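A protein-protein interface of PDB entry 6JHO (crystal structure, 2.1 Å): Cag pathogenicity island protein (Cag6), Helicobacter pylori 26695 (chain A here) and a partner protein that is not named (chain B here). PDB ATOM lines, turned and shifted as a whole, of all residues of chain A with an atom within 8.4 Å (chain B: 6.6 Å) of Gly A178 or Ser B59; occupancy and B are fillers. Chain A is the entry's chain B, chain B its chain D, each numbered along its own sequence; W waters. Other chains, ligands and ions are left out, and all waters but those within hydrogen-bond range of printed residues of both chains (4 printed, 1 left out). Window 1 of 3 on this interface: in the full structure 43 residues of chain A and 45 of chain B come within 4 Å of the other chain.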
ATOM      1  N   VAL A  86     -18.934  18.829 -32.967  1.00  0.00           N
ATOM      2  CA  VAL A  86     -18.713  17.617 -32.183  1.00  0.00           C
ATOM      3  C   VAL A  86     -19.871  16.658 -32.371  1.00  0.00           C
ATOM      4  O   VAL A  86     -19.676  15.452 -32.543  1.00  0.00           O
ATOM      5  CB  VAL A  86     -18.523  17.934 -30.688  1.00  0.00           C
ATOM      6  CG1 VAL A  86     -18.358  16.635 -29.905  1.00  0.00           C
ATOM      7  CG2 VAL A  86     -17.308  18.778 -30.463  1.00  0.00           C
ATOM      8  N   PHE A 121     -11.899  11.403 -36.344  1.00  0.00           N
ATOM      9  CA  PHE A 121     -12.732  12.194 -35.444  1.00  0.00           C
ATOM     10  C   PHE A 121     -11.862  13.052 -34.530  1.00  0.00           C
ATOM     11  O   PHE A 121     -12.098  14.258 -34.368  1.00  0.00           O
ATOM     12  CB  PHE A 121     -13.631  11.283 -34.611  1.00  0.00           C
ATOM     13  CG  PHE A 121     -14.285  11.982 -33.450  1.00  0.00           C
ATOM     14  CD1 PHE A 121     -15.485  12.656 -33.624  1.00  0.00           C
ATOM     15  CD2 PHE A 121     -13.703  11.961 -32.185  1.00  0.00           C
ATOM     16  CE1 PHE A 121     -16.088  13.325 -32.562  1.00  0.00           C
ATOM     17  CE2 PHE A 121     -14.303  12.609 -31.102  1.00  0.00           C
ATOM     18  CZ  PHE A 121     -15.505  13.294 -31.297  1.00  0.00           C
ATOM     19  N   ASN A 122     -10.834  12.437 -33.939  1.00  0.00           N
ATOM     20  CA  ASN A 122     -10.022  13.116 -32.933  1.00  0.00           C
ATOM     21  C   ASN A 122      -9.259  14.290 -33.545  1.00  0.00           C
ATOM     22  O   ASN A 122      -9.280  15.410 -33.016  1.00  0.00           O
ATOM     23  CB  ASN A 122      -9.063  12.106 -32.302  1.00  0.00           C
ATOM     24  CG  ASN A 122      -8.650  12.476 -30.882  1.00  0.00           C
ATOM     25  OD1 ASN A 122      -9.330  13.251 -30.178  1.00  0.00           O
ATOM     26  ND2 ASN A 122      -7.524  11.903 -30.447  1.00  0.00           N
ATOM     27  N   MET A 125     -11.750  17.176 -34.810  1.00  0.00           N
ATOM     28  CA  MET A 125     -12.256  18.006 -33.720  1.00  0.00           C
ATOM     29  C   MET A 125     -11.140  18.829 -33.076  1.00  0.00           C
ATOM     30  O   MET A 125     -11.297  20.031 -32.839  1.00  0.00           O
ATOM     31  CB  MET A 125     -12.953  17.133 -32.668  1.00  0.00           C
ATOM     32  CG  MET A 125     -14.383  16.733 -33.026  1.00  0.00           C
ATOM     33  SD  MET A 125     -15.394  18.043 -33.772  1.00  0.00           S
ATOM     34  CE  MET A 125     -15.064  19.487 -32.739  1.00  0.00           C
ATOM     35  N   CYS A 126      -9.999  18.200 -32.799  1.00  0.00           N
ATOM     36  CA  CYS A 126      -8.893  18.924 -32.172  1.00  0.00           C
ATOM     37  C   CYS A 126      -8.377  20.054 -33.063  1.00  0.00           C
ATOM     38  O   CYS A 126      -8.095  21.149 -32.564  1.00  0.00           O
ATOM     39  CB  CYS A 126      -7.767  17.953 -31.807  1.00  0.00           C
ATOM     40  SG  CYS A 126      -8.170  16.962 -30.360  1.00  0.00           S
ATOM     41  N   ASN A 171     -12.948  23.891 -21.820  1.00  0.00           N
ATOM     42  CA  ASN A 171     -12.789  22.713 -20.961  1.00  0.00           C
ATOM     43  C   ASN A 171     -13.920  21.716 -21.179  1.00  0.00           C
ATOM     44  O   ASN A 171     -13.696  20.500 -21.162  1.00  0.00           O
ATOM     45  CB  ASN A 171     -12.785  23.096 -19.472  1.00  0.00           C
ATOM     46  CG  ASN A 171     -11.527  23.842 -19.013  1.00  0.00           C
ATOM     47  OD1 ASN A 171     -11.521  24.365 -17.905  1.00  0.00           O
ATOM     48  ND2 ASN A 171     -10.471  23.873 -19.825  1.00  0.00           N
ATOM     49  N   GLU A 172     -15.156  22.214 -21.308  1.00  0.00           N
ATOM     50  CA  GLU A 172     -16.297  21.326 -21.498  1.00  0.00           C
ATOM     51  C   GLU A 172     -16.220  20.623 -22.841  1.00  0.00           C
ATOM     52  O   GLU A 172     -16.464  19.413 -22.932  1.00  0.00           O
ATOM     53  CB  GLU A 172     -17.615  22.103 -21.390  1.00  0.00           C
ATOM     54  CG  GLU A 172     -17.968  22.601 -19.982  1.00  0.00           C
ATOM     55  CD  GLU A 172     -17.945  21.506 -18.910  1.00  0.00           C
ATOM     56  OE1 GLU A 172     -18.693  20.495 -19.035  1.00  0.00           O
ATOM     57  OE2 GLU A 172     -17.185  21.668 -17.924  1.00  0.00           O
ATOM     58  N   ILE A 173     -15.865  21.359 -23.890  1.00  0.00           N
ATOM     59  CA  ILE A 173     -15.797  20.775 -25.229  1.00  0.00           C
ATOM     60  C   ILE A 173     -14.646  19.774 -25.330  1.00  0.00           C
ATOM     61  O   ILE A 173     -14.796  18.686 -25.900  1.00  0.00           O
ATOM     62  CB  ILE A 173     -15.671  21.886 -26.279  1.00  0.00           C
ATOM     63  CG1 ILE A 173     -16.919  22.775 -26.206  1.00  0.00           C
ATOM     64  CG2 ILE A 173     -15.559  21.283 -27.672  1.00  0.00           C
ATOM     65  CD1 ILE A 173     -16.949  23.869 -27.226  1.00  0.00           C
ATOM     66  N   VAL A 174     -13.480  20.130 -24.798  1.00  0.00           N
ATOM     67  CA  VAL A 174     -12.342  19.214 -24.855  1.00  0.00           C
ATOM     68  C   VAL A 174     -12.649  17.928 -24.087  1.00  0.00           C
ATOM     69  O   VAL A 174     -12.315  16.821 -24.542  1.00  0.00           O
ATOM     70  CB  VAL A 174     -11.067  19.908 -24.332  1.00  0.00           C
ATOM     71  CG1 VAL A 174      -9.911  18.900 -24.190  1.00  0.00           C
ATOM     72  CG2 VAL A 174     -10.660  21.045 -25.274  1.00  0.00           C
ATOM     73  N   GLN A 175     -13.293  18.045 -22.917  1.00  0.00           N
ATOM     74  CA  GLN A 175     -13.637  16.846 -22.158  1.00  0.00           C
ATOM     75  C   GLN A 175     -14.606  15.969 -22.940  1.00  0.00           C
ATOM     76  O   GLN A 175     -14.438  14.749 -22.990  1.00  0.00           O
ATOM     77  CB  GLN A 175     -14.238  17.209 -20.793  1.00  0.00           C
ATOM     78  CG  GLN A 175     -14.740  15.997 -19.989  1.00  0.00           C
ATOM     79  CD  GLN A 175     -15.480  16.391 -18.696  1.00  0.00           C
ATOM     80  OE1 GLN A 175     -15.201  17.434 -18.093  1.00  0.00           O
ATOM     81  NE2 GLN A 175     -16.445  15.567 -18.296  1.00  0.00           N
ATOM     82  N   ASP A 176     -15.619  16.583 -23.557  1.00  0.00           N
ATOM     83  CA  ASP A 176     -16.602  15.851 -24.351  1.00  0.00           C
ATOM     84  C   ASP A 176     -15.940  15.154 -25.538  1.00  0.00           C
ATOM     85  O   ASP A 176     -16.200  13.970 -25.797  1.00  0.00           O
ATOM     86  CB  ASP A 176     -17.700  16.823 -24.816  1.00  0.00           C
ATOM     87  CG  ASP A 176     -18.865  16.128 -25.529  1.00  0.00           C
ATOM     88  OD1 ASP A 176     -19.279  15.026 -25.117  1.00  0.00           O
ATOM     89  OD2 ASP A 176     -19.388  16.701 -26.506  1.00  0.00           O
ATOM     90  N   ILE A 177     -15.073  15.872 -26.262  1.00  0.00           N
ATOM     91  CA  ILE A 177     -14.303  15.257 -27.337  1.00  0.00           C
ATOM     92  C   ILE A 177     -13.505  14.078 -26.801  1.00  0.00           C
ATOM     93  O   ILE A 177     -13.444  13.010 -27.425  1.00  0.00           O
ATOM     94  CB  ILE A 177     -13.383  16.303 -27.992  1.00  0.00           C
ATOM     95  CG1 ILE A 177     -14.200  17.344 -28.739  1.00  0.00           C
ATOM     96  CG2 ILE A 177     -12.368  15.632 -28.930  1.00  0.00           C
ATOM     97  CD1 ILE A 177     -13.380  18.568 -29.133  1.00  0.00           C
ATOM     98  N   GLY A 178     -12.889  14.251 -25.630  1.00  0.00           N
ATOM     99  CA  GLY A 178     -12.070  13.189 -25.063  1.00  0.00           C
ATOM    100  C   GLY A 178     -12.859  11.925 -24.776  1.00  0.00           C
ATOM    101  O   GLY A 178     -12.433  10.817 -25.118  1.00  0.00           O
ATOM    102  N   THR A 179     -14.012  12.071 -24.122  1.00  0.00           N
ATOM    103  CA  THR A 179     -14.857  10.914 -23.836  1.00  0.00           C
ATOM    104  C   THR A 179     -15.314  10.243 -25.126  1.00  0.00           C
ATOM    105  O   THR A 179     -15.234   9.018 -25.264  1.00  0.00           O
ATOM    106  CB  THR A 179     -16.060  11.352 -22.993  1.00  0.00           C
ATOM    107  OG1 THR A 179     -15.579  11.849 -21.747  1.00  0.00           O
ATOM    108  CG2 THR A 179     -17.033  10.181 -22.730  1.00  0.00           C
ATOM    109  N   LYS A 180     -15.779  11.041 -26.092  1.00  0.00           N
ATOM    110  CA  LYS A 180     -16.250  10.503 -27.364  1.00  0.00           C
ATOM    111  C   LYS A 180     -15.137   9.770 -28.112  1.00  0.00           C
ATOM    112  O   LYS A 180     -15.375   8.734 -28.744  1.00  0.00           O
ATOM    113  CB  LYS A 180     -16.840  11.639 -28.219  1.00  0.00           C
ATOM    114  CG  LYS A 180     -18.289  12.041 -27.773  1.00  0.00           C
ATOM    115  CD  LYS A 180     -18.738  13.308 -28.502  1.00  0.00           C
ATOM    116  CE  LYS A 180     -20.261  13.560 -28.367  1.00  0.00           C
ATOM    117  NZ  LYS A 180     -20.669  13.649 -26.929  1.00  0.00           N
ATOM    118  N   TYR A 181     -13.922  10.297 -28.064  1.00  0.00           N
ATOM    119  CA  TYR A 181     -12.823   9.614 -28.727  1.00  0.00           C
ATOM    120  C   TYR A 181     -12.470   8.307 -28.008  1.00  0.00           C
ATOM    121  O   TYR A 181     -12.123   7.309 -28.649  1.00  0.00           O
ATOM    122  CB  TYR A 181     -11.605  10.532 -28.807  1.00  0.00           C
ATOM    123  CG  TYR A 181     -10.407   9.733 -29.238  1.00  0.00           C
ATOM    124  CD1 TYR A 181     -10.325   9.233 -30.546  1.00  0.00           C
ATOM    125  CD2 TYR A 181      -9.397   9.406 -28.332  1.00  0.00           C
ATOM    126  CE1 TYR A 181      -9.234   8.450 -30.957  1.00  0.00           C
ATOM    127  CE2 TYR A 181      -8.293   8.628 -28.737  1.00  0.00           C
ATOM    128  CZ  TYR A 181      -8.231   8.146 -30.040  1.00  0.00           C
ATOM    129  OH  TYR A 181      -7.161   7.355 -30.427  1.00  0.00           O
ATOM    130  N   ILE A 182     -12.534   8.299 -26.676  1.00  0.00           N
ATOM    131  CA  ILE A 182     -12.307   7.059 -25.935  1.00  0.00           C
ATOM    132  C   ILE A 182     -13.337   6.000 -26.330  1.00  0.00           C
ATOM    133  O   ILE A 182     -12.995   4.826 -26.521  1.00  0.00           O
ATOM    134  CB  ILE A 182     -12.307   7.335 -24.418  1.00  0.00           C
ATOM    135  CG1 ILE A 182     -11.006   8.042 -24.023  1.00  0.00           C
ATOM    136  CG2 ILE A 182     -12.483   6.029 -23.622  1.00  0.00           C
ATOM    137  CD1 ILE A 182     -11.097   8.827 -22.690  1.00  0.00           C
ATOM    138  N   ILE A 183     -14.599   6.403 -26.497  1.00  0.00           N
ATOM    139  CA  ILE A 183     -15.636   5.458 -26.920  1.00  0.00           C
ATOM    140  C   ILE A 183     -15.383   4.995 -28.350  1.00  0.00           C
ATOM    141  O   ILE A 183     -15.413   3.790 -28.653  1.00  0.00           O
ATOM    142  CB  ILE A 183     -17.028   6.104 -26.791  1.00  0.00           C
ATOM    143  CG1 ILE A 183     -17.420   6.248 -25.321  1.00  0.00           C
ATOM    144  CG2 ILE A 183     -18.057   5.311 -27.591  1.00  0.00           C
ATOM    145  CD1 ILE A 183     -18.416   7.364 -25.074  1.00  0.00           C
ATOM    146  N   LEU A 184     -15.113   5.942 -29.252  1.00  0.00           N
ATOM    147  CA  LEU A 184     -15.004   5.574 -30.662  1.00  0.00           C
ATOM    148  C   LEU A 184     -13.782   4.701 -30.913  1.00  0.00           C
ATOM    149  O   LEU A 184     -13.835   3.784 -31.736  1.00  0.00           O
ATOM    150  CB  LEU A 184     -14.954   6.820 -31.541  1.00  0.00           C
ATOM    151  CG  LEU A 184     -16.240   7.644 -31.670  1.00  0.00           C
ATOM    152  CD1 LEU A 184     -15.925   8.932 -32.402  1.00  0.00           C
ATOM    153  CD2 LEU A 184     -17.328   6.847 -32.442  1.00  0.00           C
ATOM    154  N   SER A 185     -12.669   4.971 -30.221  1.00  0.00           N
ATOM    155  CA  SER A 185     -11.427   4.247 -30.472  1.00  0.00           C
ATOM    156  C   SER A 185     -11.310   2.969 -29.654  1.00  0.00           C
ATOM    157  O   SER A 185     -10.354   2.207 -29.857  1.00  0.00           O
ATOM    158  CB  SER A 185     -10.223   5.140 -30.156  1.00  0.00           C
ATOM    159  OG  SER A 185     -10.139   5.332 -28.756  1.00  0.00           O
ATOM    160  N   ASN A 187     -10.299   2.955 -26.808  1.00  0.00           N
ATOM    161  CA  ASN A 187      -9.133   3.197 -25.972  1.00  0.00           C
ATOM    162  C   ASN A 187      -7.900   2.436 -26.464  1.00  0.00           C
ATOM    163  O   ASN A 187      -6.958   2.210 -25.693  1.00  0.00           O
ATOM    164  CB  ASN A 187      -9.435   2.822 -24.518  1.00  0.00           C
ATOM    165  CG  ASN A 187      -9.101   3.913 -23.545  1.00  0.00           C
ATOM    166  OD1 ASN A 187      -8.609   4.993 -23.910  1.00  0.00           O
ATOM    167  ND2 ASN A 187      -9.360   3.639 -22.283  1.00  0.00           N
ATOM    168  N   ASP B  27      -8.101   5.791 -14.285  1.00  0.00           N
ATOM    169  CA  ASP B  27      -7.834   4.731 -15.263  1.00  0.00           C
ATOM    170  C   ASP B  27      -6.983   5.279 -16.400  1.00  0.00           C
ATOM    171  O   ASP B  27      -7.501   5.918 -17.318  1.00  0.00           O
ATOM    172  CB  ASP B  27      -9.148   4.162 -15.777  1.00  0.00           C
ATOM    173  CG  ASP B  27      -9.939   3.494 -14.675  1.00  0.00           C
ATOM    174  OD1 ASP B  27      -9.321   2.731 -13.907  1.00  0.00           O
ATOM    175  OD2 ASP B  27     -11.150   3.762 -14.552  1.00  0.00           O
ATOM    176  N   ASP B  57     -14.407   7.146 -17.649  1.00  0.00           N
ATOM    177  CA  ASP B  57     -13.345   7.279 -18.634  1.00  0.00           C
ATOM    178  C   ASP B  57     -12.313   8.301 -18.171  1.00  0.00           C
ATOM    179  O   ASP B  57     -12.592   9.174 -17.337  1.00  0.00           O
ATOM    180  CB  ASP B  57     -13.915   7.722 -19.984  1.00  0.00           C
ATOM    181  CG  ASP B  57     -14.554   9.092 -19.907  1.00  0.00           C
ATOM    182  OD1 ASP B  57     -15.674   9.188 -19.361  1.00  0.00           O
ATOM    183  OD2 ASP B  57     -13.922  10.075 -20.343  1.00  0.00           O
ATOM    184  N   PHE B  58     -11.123   8.219 -18.768  1.00  0.00           N
ATOM    185  CA  PHE B  58     -10.022   9.067 -18.328  1.00  0.00           C
ATOM    186  C   PHE B  58     -10.340  10.549 -18.510  1.00  0.00           C
ATOM    187  O   PHE B  58      -9.987  11.370 -17.657  1.00  0.00           O
ATOM    188  CB  PHE B  58      -8.745   8.715 -19.091  1.00  0.00           C
ATOM    189  CG  PHE B  58      -7.585   9.609 -18.757  1.00  0.00           C
ATOM    190  CD1 PHE B  58      -6.855   9.414 -17.598  1.00  0.00           C
ATOM    191  CD2 PHE B  58      -7.225  10.645 -19.594  1.00  0.00           C
ATOM    192  CE1 PHE B  58      -5.763  10.242 -17.290  1.00  0.00           C
ATOM    193  CE2 PHE B  58      -6.152  11.476 -19.279  1.00  0.00           C
ATOM    194  CZ  PHE B  58      -5.424  11.266 -18.136  1.00  0.00           C
ATOM    195  N   SER B  59     -10.973  10.914 -19.628  1.00  0.00           N
ATOM    196  CA  SER B  59     -11.299  12.318 -19.865  1.00  0.00           C
ATOM    197  C   SER B  59     -12.162  12.877 -18.737  1.00  0.00           C
ATOM    198  O   SER B  59     -11.813  13.890 -18.117  1.00  0.00           O
ATOM    199  CB  SER B  59     -11.995  12.475 -21.215  1.00  0.00           C
ATOM    200  OG  SER B  59     -12.194  13.849 -21.511  1.00  0.00           O
ATOM    201  N   THR B  60     -13.273  12.200 -18.427  1.00  0.00           N
ATOM    202  CA  THR B  60     -14.130  12.644 -17.327  1.00  0.00           C
ATOM    203  C   THR B  60     -13.370  12.672 -16.001  1.00  0.00           C
ATOM    204  O   THR B  60     -13.449  13.647 -15.236  1.00  0.00           O
ATOM    205  CB  THR B  60     -15.351  11.729 -17.228  1.00  0.00           C
ATOM    206  OG1 THR B  60     -16.010  11.673 -18.498  1.00  0.00           O
ATOM    207  CG2 THR B  60     -16.326  12.239 -16.181  1.00  0.00           C
ATOM    208  N   GLN B  61     -12.626  11.605 -15.707  1.00  0.00           N
ATOM    209  CA  GLN B  61     -11.948  11.519 -14.414  1.00  0.00           C
ATOM    210  C   GLN B  61     -10.930  12.633 -14.230  1.00  0.00           C
ATOM    211  O   GLN B  61     -10.815  13.208 -13.142  1.00  0.00           O
ATOM    212  CB  GLN B  61     -11.264  10.165 -14.267  1.00  0.00           C
ATOM    213  CG  GLN B  61     -12.205   8.985 -14.214  1.00  0.00           C
ATOM    214  CD  GLN B  61     -11.443   7.680 -14.405  1.00  0.00           C
ATOM    215  OE1 GLN B  61     -10.243   7.695 -14.651  1.00  0.00           O
ATOM    216  NE2 GLN B  61     -12.134   6.560 -14.304  1.00  0.00           N
ATOM    217  N   ILE B  62     -10.180  12.962 -15.278  1.00  0.00           N
ATOM    218  CA  ILE B  62      -9.057  13.869 -15.087  1.00  0.00           C
ATOM    219  C   ILE B  62      -9.529  15.321 -15.019  1.00  0.00           C
ATOM    220  O   ILE B  62      -8.986  16.123 -14.253  1.00  0.00           O
ATOM    221  CB  ILE B  62      -7.996  13.641 -16.179  1.00  0.00           C
ATOM    222  CG1 ILE B  62      -6.622  13.984 -15.619  1.00  0.00           C
ATOM    223  CG2 ILE B  62      -8.297  14.447 -17.466  1.00  0.00           C
ATOM    224  CD1 ILE B  62      -6.199  13.061 -14.466  1.00  0.00           C
ATOM    225  N   PHE B  63     -10.562  15.684 -15.788  1.00  0.00           N
ATOM    226  CA  PHE B  63     -11.140  17.010 -15.626  1.00  0.00           C
ATOM    227  C   PHE B  63     -11.838  17.135 -14.274  1.00  0.00           C
ATOM    228  O   PHE B  63     -11.795  18.199 -13.652  1.00  0.00           O
ATOM    229  CB  PHE B  63     -12.100  17.304 -16.784  1.00  0.00           C
ATOM    230  CG  PHE B  63     -11.427  17.900 -17.996  1.00  0.00           C
ATOM    231  CD1 PHE B  63     -11.150  19.256 -18.054  1.00  0.00           C
ATOM    232  CD2 PHE B  63     -11.063  17.096 -19.072  1.00  0.00           C
ATOM    233  CE1 PHE B  63     -10.542  19.815 -19.181  1.00  0.00           C
ATOM    234  CE2 PHE B  63     -10.453  17.635 -20.198  1.00  0.00           C
ATOM    235  CZ  PHE B  63     -10.189  19.008 -20.252  1.00  0.00           C
ATOM    236  N   GLY B  64     -12.445  16.048 -13.792  1.00  0.00           N
ATOM    237  CA  GLY B  64     -13.040  16.065 -12.467  1.00  0.00           C
ATOM    238  C   GLY B  64     -12.012  16.211 -11.359  1.00  0.00           C
ATOM    239  O   GLY B  64     -12.229  16.949 -10.397  1.00  0.00           O
ATOM    240  N   ARG B  97       0.178  10.329 -19.221  1.00  0.00           N
ATOM    241  CA  ARG B  97      -0.514   9.199 -19.834  1.00  0.00           C
ATOM    242  C   ARG B  97       0.053   8.877 -21.212  1.00  0.00           C
ATOM    243  O   ARG B  97       0.233   7.705 -21.560  1.00  0.00           O
ATOM    244  CB  ARG B  97      -2.007   9.504 -19.933  1.00  0.00           C
ATOM    245  CG  ARG B  97      -2.864   8.351 -20.467  1.00  0.00           C
ATOM    246  CD  ARG B  97      -4.330   8.734 -20.345  1.00  0.00           C
ATOM    247  NE  ARG B  97      -5.274   7.719 -20.802  1.00  0.00           N
ATOM    248  CZ  ARG B  97      -6.102   7.891 -21.834  1.00  0.00           C
ATOM    249  NH1 ARG B  97      -6.067   9.024 -22.546  1.00  0.00           N
ATOM    250  NH2 ARG B  97      -6.948   6.927 -22.170  1.00  0.00           N
ATOM    251  N   ALA B 168      -5.361  15.352 -28.292  1.00  0.00           N
ATOM    252  CA  ALA B 168      -5.950  16.173 -27.240  1.00  0.00           C
ATOM    253  C   ALA B 168      -4.878  16.889 -26.423  1.00  0.00           C
ATOM    254  O   ALA B 168      -5.060  18.046 -26.030  1.00  0.00           O
ATOM    255  CB  ALA B 168      -6.816  15.325 -26.312  1.00  0.00           C
HETATM  256  O   HOH W   1     -10.572   5.829 -20.074  1.00  0.00           O
HETATM  257  O   HOH W   2      -7.768   5.124 -20.027  1.00  0.00           O
HETATM  258  O   HOH W   3      -6.335  12.488 -27.825  1.00  0.00           O
HETATM  259  O   HOH W   4     -17.373  13.561 -20.856  1.00  0.00           O
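O of Gln A175 is in hydrogen-bond range of OG of Ser B59 (2.8 Å).
OG1 of Thr A179 is in hydrogen-bond range of OD2 of Asp B57.
The side-chain hydroxyl (OG1) of Thr A179 lies within hydrogen-bond range of the side-chain hydroxyl (OG1) of Thr B60 (3.3 Å).
The side-chain amide oxygen (OD1) of Asn A187 is in hydrogen-bond range of the guanidinium group (NH2) of Arg B97 (3.1 Å).
O of Asn A122 sits close to SG of Cys A126 (3.3 Å).
The backbone carbonyl oxygen of Gln A175 is in hydrogen-bond range of the side-chain hydroxyl of Thr A179 (3.4 Å).
The backbone carbonyl oxygen of Ile A182 lies within hydrogen-bond range of the backbone NH of Asn A187, at 3.3 Å.
OG of Ser A185 lies close to N of Asn A187 (3.1 Å).
N of Ser B59 lies within hydrogen-bond range of OD2 of Asp B57, 3.1 Å away.
The side-chain carboxylate of Asp B57 is in hydrogen-bond range of the side-chain hydroxyl of Thr B60 (2.7 Å).
Cys A126 touches Ala B168.
O of Asn A171 touches CE1 of Phe B63, 3.8 Å away.
CG1 of Val A174 touches CZ of Phe B63 (3.9 Å).
Gln A175 touches Thr B60.
Phe B63 touches Gln A175 (CB to OE1, 3.4 Å).
Gly A178 touches Ser B59 (CA to OG, 3.6 Å).
N of Thr A179 touches CB of Ser B59, 3.6 Å away.
Ile A182 touches Asp B57 (CD1 to OD2, 3.9 Å).
Ile A182 touches Phe B58 (CD1 to N, 3.97 Å).
Ile A182 touches Ser B59.
Asp A176 touches none of the printed residues of chain B.
Gly A178 touches one residue of chain B.
Of the printed residues of chain B, Thr A179 touches Asp B57, Ser B59 and Thr B60.
Printed residues of chain B within 4 Å of Asn A187: Arg B97 (3.1 Å).
Of chain A, only Gln A175, Gly A178, Thr A179 and Ile A182 come within 4 Å of Ser B59.
Of the printed residues of chain A, Ala B168 touches Cys A126 (3.8 Å).
Of the 21 printed residues of chain A, 8 touch a printed residue of chain B.
Of the 11 printed residues of chain B, 7 touch a printed residue of chain A.
Hydrophobic or aromatic side chains of chain B within 4 Å of the printed part of chain A: Phe B63.
Among the printed residues, 14 pairs touch across the chains.
Among the printed residues, no Asp or Glu carboxylate lies within 4 Å of a Lys or Arg side-chain nitrogen of the other chain.
Water W4 lies within hydrogen-bond range of the side-chain hydroxyl of Thr A179 (2.6 Å), the side-chain hydroxyl of Thr B60 (3.3 Å) and the side-chain amide nitrogen of Gln A175 (3.4 Å).
Water W1 lies within hydrogen-bond range of the backbone NH of Phe B58 (2.8 Å) and the side-chain amide nitrogen of Asn A187 (3.3 Å).
Water W2 lies within hydrogen-bond range of the backbone carbonyl oxygen of Asp B27 (2.8 Å), the guanidinium group of Arg B97 (2.9 Å) and the side-chain amide nitrogen of Asn A187 (3.1 Å).
Water W3 lies within hydrogen-bond range of ND2 of Asn A122 (2.9 Å) and N of Ala B168 (3.1 Å).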
